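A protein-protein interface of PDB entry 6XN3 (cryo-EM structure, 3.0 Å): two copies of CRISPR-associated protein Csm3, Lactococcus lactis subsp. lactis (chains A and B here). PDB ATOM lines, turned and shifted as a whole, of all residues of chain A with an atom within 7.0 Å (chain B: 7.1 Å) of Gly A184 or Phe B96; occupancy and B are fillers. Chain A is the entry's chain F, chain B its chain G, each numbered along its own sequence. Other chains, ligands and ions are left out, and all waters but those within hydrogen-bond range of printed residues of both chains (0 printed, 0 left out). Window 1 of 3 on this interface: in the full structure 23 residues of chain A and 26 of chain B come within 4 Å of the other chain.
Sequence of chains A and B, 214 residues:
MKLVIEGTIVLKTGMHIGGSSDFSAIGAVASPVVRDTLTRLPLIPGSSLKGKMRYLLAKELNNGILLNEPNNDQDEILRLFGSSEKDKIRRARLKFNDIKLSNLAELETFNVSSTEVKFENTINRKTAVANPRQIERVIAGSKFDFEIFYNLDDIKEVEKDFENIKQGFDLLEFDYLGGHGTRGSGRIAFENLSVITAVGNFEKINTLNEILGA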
ATOM      1  N   THR A  13       2.956   4.179  11.216  1.00  0.00           N
ATOM      2  CA  THR A  13       2.504   5.316  12.005  1.00  0.00           C
ATOM      3  C   THR A  13       3.726   6.184  12.269  1.00  0.00           C
ATOM      4  O   THR A  13       4.729   6.107  11.559  1.00  0.00           O
ATOM      5  CB  THR A  13       1.836   4.909  13.326  1.00  0.00           C
ATOM      6  OG1 THR A  13       2.758   4.155  14.119  1.00  0.00           O
ATOM      7  CG2 THR A  13       0.565   4.108  13.112  1.00  0.00           C
ATOM      8  N   GLY A  14       3.630   7.038  13.274  1.00  0.00           N
ATOM      9  CA  GLY A  14       4.644   8.032  13.551  1.00  0.00           C
ATOM     10  C   GLY A  14       6.071   7.646  13.896  1.00  0.00           C
ATOM     11  O   GLY A  14       6.973   8.019  13.149  1.00  0.00           O
ATOM     12  N   MET A  15       6.295   6.931  15.004  1.00  0.00           N
ATOM     13  CA  MET A  15       7.629   6.603  15.531  1.00  0.00           C
ATOM     14  C   MET A  15       8.398   7.889  15.856  1.00  0.00           C
ATOM     15  O   MET A  15       9.176   8.414  15.074  1.00  0.00           O
ATOM     16  CB  MET A  15       8.391   5.643  14.594  1.00  0.00           C
ATOM     17  CG  MET A  15       9.771   5.117  15.003  1.00  0.00           C
ATOM     18  SD  MET A  15      11.226   6.132  14.730  1.00  0.00           S
ATOM     19  CE  MET A  15      11.375   6.045  12.969  1.00  0.00           C
ATOM     20  N   LYS A 118       3.274  16.752  15.339  1.00  0.00           N
ATOM     21  CA  LYS A 118       1.957  16.321  15.778  1.00  0.00           C
ATOM     22  C   LYS A 118       1.490  17.219  16.909  1.00  0.00           C
ATOM     23  O   LYS A 118       2.225  17.456  17.869  1.00  0.00           O
ATOM     24  CB  LYS A 118       1.967  14.868  16.232  1.00  0.00           C
ATOM     25  CG  LYS A 118       0.575  14.302  16.353  1.00  0.00           C
ATOM     26  CD  LYS A 118       0.558  13.036  17.149  1.00  0.00           C
ATOM     27  CE  LYS A 118      -0.795  12.384  17.071  1.00  0.00           C
ATOM     28  NZ  LYS A 118      -1.281  12.006  18.417  1.00  0.00           N
ATOM     29  N   ARG A 137       7.831  14.228  14.927  1.00  0.00           N
ATOM     30  CA  ARG A 137       7.547  12.823  14.722  1.00  0.00           C
ATOM     31  C   ARG A 137       7.911  12.499  13.285  1.00  0.00           C
ATOM     32  O   ARG A 137       7.731  13.345  12.409  1.00  0.00           O
ATOM     33  CB  ARG A 137       6.070  12.558  15.018  1.00  0.00           C
ATOM     34  CG  ARG A 137       5.733  11.139  15.279  1.00  0.00           C
ATOM     35  CD  ARG A 137       4.260  10.940  15.567  1.00  0.00           C
ATOM     36  NE  ARG A 137       3.476  11.090  14.351  1.00  0.00           N
ATOM     37  CZ  ARG A 137       2.171  10.869  14.268  1.00  0.00           C
ATOM     38  NH1 ARG A 137       1.509  10.425  15.318  1.00  0.00           N
ATOM     39  NH2 ARG A 137       1.543  11.038  13.117  1.00  0.00           N
ATOM     40  N   HIS A 180       5.502   7.555  22.254  1.00  0.00           N
ATOM     41  CA  HIS A 180       4.128   7.467  22.725  1.00  0.00           C
ATOM     42  C   HIS A 180       3.312   6.481  21.913  1.00  0.00           C
ATOM     43  O   HIS A 180       2.396   6.880  21.195  1.00  0.00           O
ATOM     44  CB  HIS A 180       3.480   8.835  22.630  1.00  0.00           C
ATOM     45  CG  HIS A 180       4.400   9.954  22.982  1.00  0.00           C
ATOM     46  ND1 HIS A 180       4.928  10.116  24.242  1.00  0.00           N
ATOM     47  CD2 HIS A 180       4.917  10.947  22.226  1.00  0.00           C
ATOM     48  CE1 HIS A 180       5.710  11.180  24.254  1.00  0.00           C
ATOM     49  NE2 HIS A 180       5.721  11.702  23.043  1.00  0.00           N
ATOM     50  N   GLY A 181       3.624   5.194  22.018  1.00  0.00           N
ATOM     51  CA  GLY A 181       3.011   4.236  21.121  1.00  0.00           C
ATOM     52  C   GLY A 181       1.595   3.886  21.515  1.00  0.00           C
ATOM     53  O   GLY A 181       0.785   3.510  20.668  1.00  0.00           O
ATOM     54  N   THR A 182       1.274   4.017  22.796  1.00  0.00           N
ATOM     55  CA  THR A 182      -0.061   3.698  23.269  1.00  0.00           C
ATOM     56  C   THR A 182      -1.097   4.689  22.750  1.00  0.00           C
ATOM     57  O   THR A 182      -2.268   4.330  22.594  1.00  0.00           O
ATOM     58  CB  THR A 182      -0.034   3.661  24.788  1.00  0.00           C
ATOM     59  OG1 THR A 182       1.095   2.891  25.203  1.00  0.00           O
ATOM     60  CG2 THR A 182      -1.250   2.988  25.327  1.00  0.00           C
ATOM     61  N   ARG A 183      -0.682   5.907  22.422  1.00  0.00           N
ATOM     62  CA  ARG A 183      -1.543   6.878  21.772  1.00  0.00           C
ATOM     63  C   ARG A 183      -1.374   6.901  20.264  1.00  0.00           C
ATOM     64  O   ARG A 183      -1.438   7.976  19.664  1.00  0.00           O
ATOM     65  CB  ARG A 183      -1.306   8.282  22.305  1.00  0.00           C
ATOM     66  CG  ARG A 183      -1.946   8.594  23.608  1.00  0.00           C
ATOM     67  CD  ARG A 183      -1.127   8.161  24.785  1.00  0.00           C
ATOM     68  NE  ARG A 183       0.207   8.736  24.703  1.00  0.00           N
ATOM     69  CZ  ARG A 183       0.507   9.973  25.066  1.00  0.00           C
ATOM     70  NH1 ARG A 183      -0.447  10.788  25.458  1.00  0.00           N
ATOM     71  NH2 ARG A 183       1.746  10.421  24.972  1.00  0.00           N
ATOM     72  N   GLY A 184      -1.132   5.760  19.641  1.00  0.00           N
ATOM     73  CA  GLY A 184      -1.121   5.741  18.198  1.00  0.00           C
ATOM     74  C   GLY A 184       0.149   6.275  17.583  1.00  0.00           C
ATOM     75  O   GLY A 184       0.137   7.315  16.923  1.00  0.00           O
ATOM     76  N   SER A 185       1.255   5.583  17.812  1.00  0.00           N
ATOM     77  CA  SER A 185       2.518   5.946  17.196  1.00  0.00           C
ATOM     78  C   SER A 185       3.398   4.714  17.160  1.00  0.00           C
ATOM     79  O   SER A 185       3.115   3.709  17.811  1.00  0.00           O
ATOM     80  CB  SER A 185       3.216   7.076  17.951  1.00  0.00           C
ATOM     81  OG  SER A 185       4.557   7.193  17.531  1.00  0.00           O
ATOM     82  N   GLY A 186       4.448   4.789  16.364  1.00  0.00           N
ATOM     83  CA  GLY A 186       5.503   3.817  16.468  1.00  0.00           C
ATOM     84  C   GLY A 186       5.260   2.489  15.804  1.00  0.00           C
ATOM     85  O   GLY A 186       6.125   1.614  15.901  1.00  0.00           O
ATOM     86  N   ARG A 187       4.129   2.290  15.143  1.00  0.00           N
ATOM     87  CA  ARG A 187       3.852   0.981  14.578  1.00  0.00           C
ATOM     88  C   ARG A 187       4.707   0.743  13.347  1.00  0.00           C
ATOM     89  O   ARG A 187       4.700   1.531  12.402  1.00  0.00           O
ATOM     90  CB  ARG A 187       2.378   0.853  14.228  1.00  0.00           C
ATOM     91  CG  ARG A 187       1.977  -0.535  13.826  1.00  0.00           C
ATOM     92  CD  ARG A 187       0.540  -0.539  13.410  1.00  0.00           C
ATOM     93  NE  ARG A 187       0.169  -1.777  12.755  1.00  0.00           N
ATOM     94  CZ  ARG A 187      -1.026  -1.996  12.233  1.00  0.00           C
ATOM     95  NH1 ARG A 187      -1.952  -1.057  12.299  1.00  0.00           N
ATOM     96  NH2 ARG A 187      -1.296  -3.153  11.650  1.00  0.00           N
ATOM     97  N   PRO B  45      -6.144  10.600  14.820  1.00  0.00           N
ATOM     98  CA  PRO B  45      -5.056  10.158  15.688  1.00  0.00           C
ATOM     99  C   PRO B  45      -5.571   9.164  16.708  1.00  0.00           C
ATOM    100  O   PRO B  45      -6.732   9.213  17.111  1.00  0.00           O
ATOM    101  CB  PRO B  45      -4.585  11.450  16.355  1.00  0.00           C
ATOM    102  CG  PRO B  45      -5.118  12.541  15.516  1.00  0.00           C
ATOM    103  CD  PRO B  45      -6.393  12.040  14.945  1.00  0.00           C
ATOM    104  N   GLY B  46      -4.699   8.243  17.113  1.00  0.00           N
ATOM    105  CA  GLY B  46      -5.070   7.308  18.158  1.00  0.00           C
ATOM    106  C   GLY B  46      -5.132   7.964  19.517  1.00  0.00           C
ATOM    107  O   GLY B  46      -5.792   7.459  20.428  1.00  0.00           O
ATOM    108  N   SER B  47      -4.445   9.096  19.667  1.00  0.00           N
ATOM    109  CA  SER B  47      -4.489   9.847  20.910  1.00  0.00           C
ATOM    110  C   SER B  47      -5.877  10.398  21.176  1.00  0.00           C
ATOM    111  O   SER B  47      -6.349  10.371  22.316  1.00  0.00           O
ATOM    112  CB  SER B  47      -3.476  10.980  20.856  1.00  0.00           C
ATOM    113  OG  SER B  47      -3.785  11.855  19.795  1.00  0.00           O
ATOM    114  N   SER B  48      -6.555  10.877  20.129  1.00  0.00           N
ATOM    115  CA  SER B  48      -7.895  11.438  20.288  1.00  0.00           C
ATOM    116  C   SER B  48      -8.896  10.369  20.683  1.00  0.00           C
ATOM    117  O   SER B  48      -9.698  10.562  21.606  1.00  0.00           O
ATOM    118  CB  SER B  48      -8.333  12.112  18.994  1.00  0.00           C
ATOM    119  OG  SER B  48      -9.637  12.632  19.126  1.00  0.00           O
ATOM    120  N   LEU B  49      -8.852   9.233  19.993  1.00  0.00           N
ATOM    121  CA  LEU B  49      -9.761   8.136  20.286  1.00  0.00           C
ATOM    122  C   LEU B  49      -9.512   7.587  21.680  1.00  0.00           C
ATOM    123  O   LEU B  49     -10.460   7.354  22.436  1.00  0.00           O
ATOM    124  CB  LEU B  49      -9.599   7.049  19.229  1.00  0.00           C
ATOM    125  CG  LEU B  49     -10.489   5.823  19.363  1.00  0.00           C
ATOM    126  CD1 LEU B  49     -11.934   6.222  19.222  1.00  0.00           C
ATOM    127  CD2 LEU B  49     -10.121   4.798  18.320  1.00  0.00           C
ATOM    128  N   LYS B  50      -8.239   7.439  22.059  1.00  0.00           N
ATOM    129  CA  LYS B  50      -7.906   6.923  23.382  1.00  0.00           C
ATOM    130  C   LYS B  50      -8.339   7.881  24.482  1.00  0.00           C
ATOM    131  O   LYS B  50      -8.897   7.456  25.496  1.00  0.00           O
ATOM    132  CB  LYS B  50      -6.408   6.650  23.483  1.00  0.00           C
ATOM    133  CG  LYS B  50      -6.020   6.041  24.806  1.00  0.00           C
ATOM    134  CD  LYS B  50      -4.548   5.779  24.911  1.00  0.00           C
ATOM    135  CE  LYS B  50      -4.212   5.335  26.310  1.00  0.00           C
ATOM    136  NZ  LYS B  50      -2.824   5.653  26.668  1.00  0.00           N
ATOM    137  N   GLY B  51      -8.111   9.179  24.286  1.00  0.00           N
ATOM    138  CA  GLY B  51      -8.473  10.144  25.310  1.00  0.00           C
ATOM    139  C   GLY B  51      -9.971  10.270  25.493  1.00  0.00           C
ATOM    140  O   GLY B  51     -10.463  10.332  26.624  1.00  0.00           O
ATOM    141  N   MET B  53     -12.281   7.950  24.680  1.00  0.00           N
ATOM    142  CA  MET B  53     -12.730   6.694  25.271  1.00  0.00           C
ATOM    143  C   MET B  53     -12.431   6.638  26.755  1.00  0.00           C
ATOM    144  O   MET B  53     -13.267   6.190  27.542  1.00  0.00           O
ATOM    145  CB  MET B  53     -12.060   5.515  24.587  1.00  0.00           C
ATOM    146  CG  MET B  53     -12.658   5.086  23.304  1.00  0.00           C
ATOM    147  SD  MET B  53     -11.952   3.492  22.922  1.00  0.00           S
ATOM    148  CE  MET B  53     -12.470   2.551  24.352  1.00  0.00           C
ATOM    149  N   ARG B  54     -11.244   7.094  27.157  1.00  0.00           N
ATOM    150  CA  ARG B  54     -10.885   7.053  28.565  1.00  0.00           C
ATOM    151  C   ARG B  54     -11.748   8.002  29.376  1.00  0.00           C
ATOM    152  O   ARG B  54     -12.193   7.647  30.470  1.00  0.00           O
ATOM    153  CB  ARG B  54      -9.407   7.380  28.756  1.00  0.00           C
ATOM    154  CG  ARG B  54      -8.973   7.327  30.205  1.00  0.00           C
ATOM    155  CD  ARG B  54      -7.483   7.352  30.362  1.00  0.00           C
ATOM    156  NE  ARG B  54      -7.113   7.249  31.763  1.00  0.00           N
ATOM    157  CZ  ARG B  54      -5.919   6.862  32.184  1.00  0.00           C
ATOM    158  NH1 ARG B  54      -4.990   6.535  31.307  1.00  0.00           N
ATOM    159  NH2 ARG B  54      -5.659   6.792  33.475  1.00  0.00           N
ATOM    160  N   LEU B  80      -6.717  -0.581  31.821  1.00  0.00           N
ATOM    161  CA  LEU B  80      -7.038  -0.551  30.401  1.00  0.00           C
ATOM    162  C   LEU B  80      -6.258   0.529  29.659  1.00  0.00           C
ATOM    163  O   LEU B  80      -5.895   0.344  28.495  1.00  0.00           O
ATOM    164  CB  LEU B  80      -8.537  -0.359  30.207  1.00  0.00           C
ATOM    165  CG  LEU B  80      -9.327  -1.659  30.321  1.00  0.00           C
ATOM    166  CD1 LEU B  80     -10.783  -1.361  30.566  1.00  0.00           C
ATOM    167  CD2 LEU B  80      -9.161  -2.493  29.077  1.00  0.00           C
ATOM    168  N   PHE B  81      -5.987   1.661  30.300  1.00  0.00           N
ATOM    169  CA  PHE B  81      -5.395   2.812  29.624  1.00  0.00           C
ATOM    170  C   PHE B  81      -4.086   3.277  30.249  1.00  0.00           C
ATOM    171  O   PHE B  81      -3.687   4.425  30.079  1.00  0.00           O
ATOM    172  CB  PHE B  81      -6.370   3.980  29.587  1.00  0.00           C
ATOM    173  CG  PHE B  81      -7.586   3.743  28.755  1.00  0.00           C
ATOM    174  CD1 PHE B  81      -8.722   3.186  29.304  1.00  0.00           C
ATOM    175  CD2 PHE B  81      -7.599   4.111  27.428  1.00  0.00           C
ATOM    176  CE1 PHE B  81      -9.839   2.979  28.535  1.00  0.00           C
ATOM    177  CE2 PHE B  81      -8.709   3.906  26.663  1.00  0.00           C
ATOM    178  CZ  PHE B  81      -9.831   3.340  27.217  1.00  0.00           C
ATOM    179  N   LEU B  94      -4.127  -1.801  26.045  1.00  0.00           N
ATOM    180  CA  LEU B  94      -4.606  -1.367  24.747  1.00  0.00           C
ATOM    181  C   LEU B  94      -3.529  -0.566  24.041  1.00  0.00           C
ATOM    182  O   LEU B  94      -2.828   0.234  24.657  1.00  0.00           O
ATOM    183  CB  LEU B  94      -5.864  -0.513  24.902  1.00  0.00           C
ATOM    184  CG  LEU B  94      -7.240  -1.158  24.791  1.00  0.00           C
ATOM    185  CD1 LEU B  94      -7.416  -2.209  25.832  1.00  0.00           C
ATOM    186  CD2 LEU B  94      -8.289  -0.096  24.989  1.00  0.00           C
ATOM    187  N   LYS B  95      -3.406  -0.781  22.737  1.00  0.00           N
ATOM    188  CA  LYS B  95      -2.470  -0.019  21.913  1.00  0.00           C
ATOM    189  C   LYS B  95      -3.287   0.576  20.775  1.00  0.00           C
ATOM    190  O   LYS B  95      -3.591  -0.110  19.801  1.00  0.00           O
ATOM    191  CB  LYS B  95      -1.340  -0.893  21.389  1.00  0.00           C
ATOM    192  CG  LYS B  95      -0.064  -0.156  21.008  1.00  0.00           C
ATOM    193  CD  LYS B  95      -0.083   0.285  19.560  1.00  0.00           C
ATOM    194  CE  LYS B  95       1.263   0.754  19.083  1.00  0.00           C
ATOM    195  NZ  LYS B  95       1.157   1.444  17.778  1.00  0.00           N
ATOM    196  N   PHE B  96      -3.636   1.846  20.902  1.00  0.00           N
ATOM    197  CA  PHE B  96      -4.375   2.499  19.842  1.00  0.00           C
ATOM    198  C   PHE B  96      -3.444   2.808  18.678  1.00  0.00           C
ATOM    199  O   PHE B  96      -2.222   2.766  18.802  1.00  0.00           O
ATOM    200  CB  PHE B  96      -5.038   3.769  20.359  1.00  0.00           C
ATOM    201  CG  PHE B  96      -6.229   3.515  21.226  1.00  0.00           C
ATOM    202  CD1 PHE B  96      -6.077   3.141  22.542  1.00  0.00           C
ATOM    203  CD2 PHE B  96      -7.503   3.651  20.720  1.00  0.00           C
ATOM    204  CE1 PHE B  96      -7.164   2.906  23.331  1.00  0.00           C
ATOM    205  CE2 PHE B  96      -8.594   3.423  21.515  1.00  0.00           C
ATOM    206  CZ  PHE B  96      -8.421   3.045  22.818  1.00  0.00           C
ATOM    207  N   ASN B  97      -4.036   3.090  17.526  1.00  0.00           N
ATOM    208  CA  ASN B  97      -3.259   3.350  16.327  1.00  0.00           C
ATOM    209  C   ASN B  97      -3.833   4.545  15.592  1.00  0.00           C
ATOM    210  O   ASN B  97      -5.014   4.863  15.719  1.00  0.00           O
ATOM    211  CB  ASN B  97      -3.230   2.141  15.401  1.00  0.00           C
ATOM    212  CG  ASN B  97      -2.371   1.039  15.934  1.00  0.00           C
ATOM    213  OD1 ASN B  97      -1.291   1.286  16.450  1.00  0.00           O
ATOM    214  ND2 ASN B  97      -2.838  -0.189  15.809  1.00  0.00           N
ATOM    215  N   ASP B  98      -2.970   5.212  14.839  1.00  0.00           N
ATOM    216  CA  ASP B  98      -3.393   6.295  13.970  1.00  0.00           C
ATOM    217  C   ASP B  98      -4.284   5.733  12.876  1.00  0.00           C
ATOM    218  O   ASP B  98      -3.863   4.864  12.107  1.00  0.00           O
ATOM    219  CB  ASP B  98      -2.173   6.983  13.375  1.00  0.00           C
ATOM    220  CG  ASP B  98      -1.630   8.071  14.272  1.00  0.00           C
ATOM    221  OD1 ASP B  98      -2.144   8.219  15.396  1.00  0.00           O
ATOM    222  OD2 ASP B  98      -0.683   8.773  13.860  1.00  0.00           O
ATOM    223  N   ILE B  99      -5.517   6.216  12.811  1.00  0.00           N
ATOM    224  CA  ILE B  99      -6.513   5.694  11.889  1.00  0.00           C
ATOM    225  C   ILE B  99      -6.518   6.551  10.636  1.00  0.00           C
ATOM    226  O   ILE B  99      -6.580   7.783  10.718  1.00  0.00           O
ATOM    227  CB  ILE B  99      -7.904   5.659  12.535  1.00  0.00           C
ATOM    228  CG1 ILE B  99      -7.803   5.228  13.992  1.00  0.00           C
ATOM    229  CG2 ILE B  99      -8.779   4.709  11.800  1.00  0.00           C
ATOM    230  CD1 ILE B  99      -9.064   5.428  14.758  1.00  0.00           C
ATOM    231  N   PHE B 146      -9.892   0.855  11.790  1.00  0.00           N
ATOM    232  CA  PHE B 146      -8.952   0.962  12.893  1.00  0.00           C
ATOM    233  C   PHE B 146      -8.573  -0.407  13.433  1.00  0.00           C
ATOM    234  O   PHE B 146      -9.332  -1.372  13.329  1.00  0.00           O
ATOM    235  CB  PHE B 146      -9.510   1.839  14.028  1.00  0.00           C
ATOM    236  CG  PHE B 146     -10.612   1.206  14.823  1.00  0.00           C
ATOM    237  CD1 PHE B 146     -11.901   1.191  14.338  1.00  0.00           C
ATOM    238  CD2 PHE B 146     -10.372   0.656  16.064  1.00  0.00           C
ATOM    239  CE1 PHE B 146     -12.920   0.628  15.070  1.00  0.00           C
ATOM    240  CE2 PHE B 146     -11.391   0.079  16.783  1.00  0.00           C
ATOM    241  CZ  PHE B 146     -12.660   0.067  16.286  1.00  0.00           C
ATOM    242  N   GLU B 147      -7.379  -0.466  14.018  1.00  0.00           N
ATOM    243  CA  GLU B 147      -6.864  -1.655  14.681  1.00  0.00           C
ATOM    244  C   GLU B 147      -6.333  -1.232  16.038  1.00  0.00           C
ATOM    245  O   GLU B 147      -5.499  -0.329  16.116  1.00  0.00           O
ATOM    246  CB  GLU B 147      -5.744  -2.300  13.864  1.00  0.00           C
ATOM    247  CG  GLU B 147      -6.174  -2.893  12.544  1.00  0.00           C
ATOM    248  CD  GLU B 147      -5.015  -3.493  11.777  1.00  0.00           C
ATOM    249  OE1 GLU B 147      -3.862  -3.333  12.222  1.00  0.00           O
ATOM    250  OE2 GLU B 147      -5.249  -4.121  10.728  1.00  0.00           O
ATOM    251  N   ILE B 148      -6.810  -1.866  17.102  1.00  0.00           N
ATOM    252  CA  ILE B 148      -6.273  -1.660  18.439  1.00  0.00           C
ATOM    253  C   ILE B 148      -5.706  -2.980  18.924  1.00  0.00           C
ATOM    254  O   ILE B 148      -6.413  -3.992  18.948  1.00  0.00           O
ATOM    255  CB  ILE B 148      -7.335  -1.145  19.419  1.00  0.00           C
ATOM    256  CG1 ILE B 148      -7.916   0.171  18.940  1.00  0.00           C
ATOM    257  CG2 ILE B 148      -6.741  -0.942  20.779  1.00  0.00           C
ATOM    258  CD1 ILE B 148      -9.233   0.462  19.573  1.00  0.00           C
ATOM    259  N   PHE B 149      -4.440  -2.970  19.315  1.00  0.00           N
ATOM    260  CA  PHE B 149      -3.813  -4.163  19.851  1.00  0.00           C
ATOM    261  C   PHE B 149      -4.147  -4.299  21.326  1.00  0.00           C
ATOM    262  O   PHE B 149      -3.894  -3.386  22.115  1.00  0.00           O
ATOM    263  CB  PHE B 149      -2.306  -4.104  19.656  1.00  0.00           C
ATOM    264  CG  PHE B 149      -1.896  -3.816  18.254  1.00  0.00           C
ATOM    265  CD1 PHE B 149      -2.425  -4.541  17.207  1.00  0.00           C
ATOM    266  CD2 PHE B 149      -0.978  -2.828  17.983  1.00  0.00           C
ATOM    267  CE1 PHE B 149      -2.048  -4.282  15.913  1.00  0.00           C
ATOM    268  CE2 PHE B 149      -0.600  -2.561  16.695  1.00  0.00           C
ATOM    269  CZ  PHE B 149      -1.135  -3.290  15.657  1.00  0.00           C
ATOM    270  N   ILE B 165     -14.815  -2.254  27.211  1.00  0.00           N
ATOM    271  CA  ILE B 165     -14.499  -1.686  25.903  1.00  0.00           C
ATOM    272  C   ILE B 165     -15.766  -1.501  25.077  1.00  0.00           C
ATOM    273  O   ILE B 165     -15.954  -0.464  24.429  1.00  0.00           O
ATOM    274  CB  ILE B 165     -13.448  -2.555  25.191  1.00  0.00           C
ATOM    275  CG1 ILE B 165     -12.068  -2.249  25.765  1.00  0.00           C
ATOM    276  CG2 ILE B 165     -13.460  -2.351  23.683  1.00  0.00           C
ATOM    277  CD1 ILE B 165     -10.962  -2.995  25.112  1.00  0.00           C
ATOM    278  N   PHE B 169     -17.375   1.988  23.760  1.00  0.00           N
ATOM    279  CA  PHE B 169     -17.796   2.139  22.373  1.00  0.00           C
ATOM    280  C   PHE B 169     -19.259   2.547  22.281  1.00  0.00           C
ATOM    281  O   PHE B 169     -19.640   3.337  21.413  1.00  0.00           O
ATOM    282  CB  PHE B 169     -17.547   0.838  21.617  1.00  0.00           C
ATOM    283  CG  PHE B 169     -16.157   0.703  21.082  1.00  0.00           C
ATOM    284  CD1 PHE B 169     -15.167   1.594  21.440  1.00  0.00           C
ATOM    285  CD2 PHE B 169     -15.829  -0.347  20.259  1.00  0.00           C
ATOM    286  CE1 PHE B 169     -13.898   1.457  20.952  1.00  0.00           C
ATOM    287  CE2 PHE B 169     -14.549  -0.486  19.789  1.00  0.00           C
ATOM    288  CZ  PHE B 169     -13.585   0.417  20.136  1.00  0.00           C
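The guanidinium group of Arg A187 is in salt-bridge range of the side-chain carboxylate of Glu B147 (2.6 Å).
The side-chain carboxylate of Asp B98 lies close to the backbone carbonyl oxygen of Gly A184 (2.9 Å).
The backbone carbonyl oxygen of Arg A183 lies within hydrogen-bond range of the backbone NH of Ser B47.
The guanidinium group (NH1) of Arg A137 is in salt-bridge range of the side-chain carboxylate (OD2) of Asp B98 (3.1 Å).
The backbone carbonyl oxygen (O) of Ser A185 is in hydrogen-bond range of the side-chain amino group (NZ) of Lys B95 (3.0 Å).
N of Gly A184 lies close to O of Phe B96 (3.3 Å).
NZ of Lys A118 sits at hydrogen-bond distance from OG of Ser B47, at 2.9 Å.
O of Thr A182 is in hydrogen-bond range of N of Phe B96, 3.3 Å away.
N of Arg A187 lies within hydrogen-bond range of OG1 of Thr A13, at 2.5 Å.
The backbone NH of Met A15 sits at hydrogen-bond distance from the side-chain hydroxyl of Ser A185, at 3.1 Å.
ND2 of Asn B97 is in hydrogen-bond range of O of Glu B147 (2.7 Å).
OD1 of Asn B97 lies within hydrogen-bond range of NZ of Lys B95 (2.8 Å).
The backbone carbonyl oxygen of Phe B149 lies within hydrogen-bond range of the backbone NH of Lys B95, at 2.7 Å.
OG1 of Thr A13 lies within hydrogen-bond range of N of Gly A186.
Thr A13 touches Asp B98.
Pro B45 touches Lys A118.
Lys B95 touches Gly A181.
Phe B96 touches Gly A181 (O to O, 3.6 Å).
NZ of Lys B50 touches CG2 of Thr A182 (3.4 Å).
Leu B94 touches Thr A182 (O to CG2, 3.2 Å).
Lys B50 touches Arg A183.
Lys B95 touches Arg A187.
Arg A187 touches Asn B97.
NE of Arg A187 touches CZ of Phe B149 (3.5 Å).
Met A15 touches none of the printed residues of chain B.
Printed residues of chain B within 4 Å of Lys A118: Pro B45 and Ser B47.
Printed residues of chain B within 4 Å of Arg A183: Gly B46, Ser B47 and Lys B50.
Of chain B, only Phe B96, Asn B97 and Asp B98 come within 4 Å of Gly A184.
Printed residues of chain A within 4 Å of Leu B94: Thr A182.
Of the printed residues of chain A, Phe B96 touches Gly A181, Thr A182 and Gly A184.
Of the printed residues of chain A, Asn B97 touches Gly A184 and Arg A187.
Of the printed residues of chain A, Asp B98 touches Thr A13 (3.98 Å), Arg A137 (3.1 Å) and Gly A184 (2.9 Å).
The nearest residue of chain A that does not touch Phe B96 is Arg A183 (4.5 Å).
Hydrophobic or aromatic side chains of chain B that line the printed part of chain A: Pro B45, Phe B96 and Phe B149.
Among the printed residues, 20 pairs touch across the chains.
No position is printed for both chains.
Of the 20 pairs that touch across the chains among the printed residues, none has its exchanged pair printed and touching as well.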
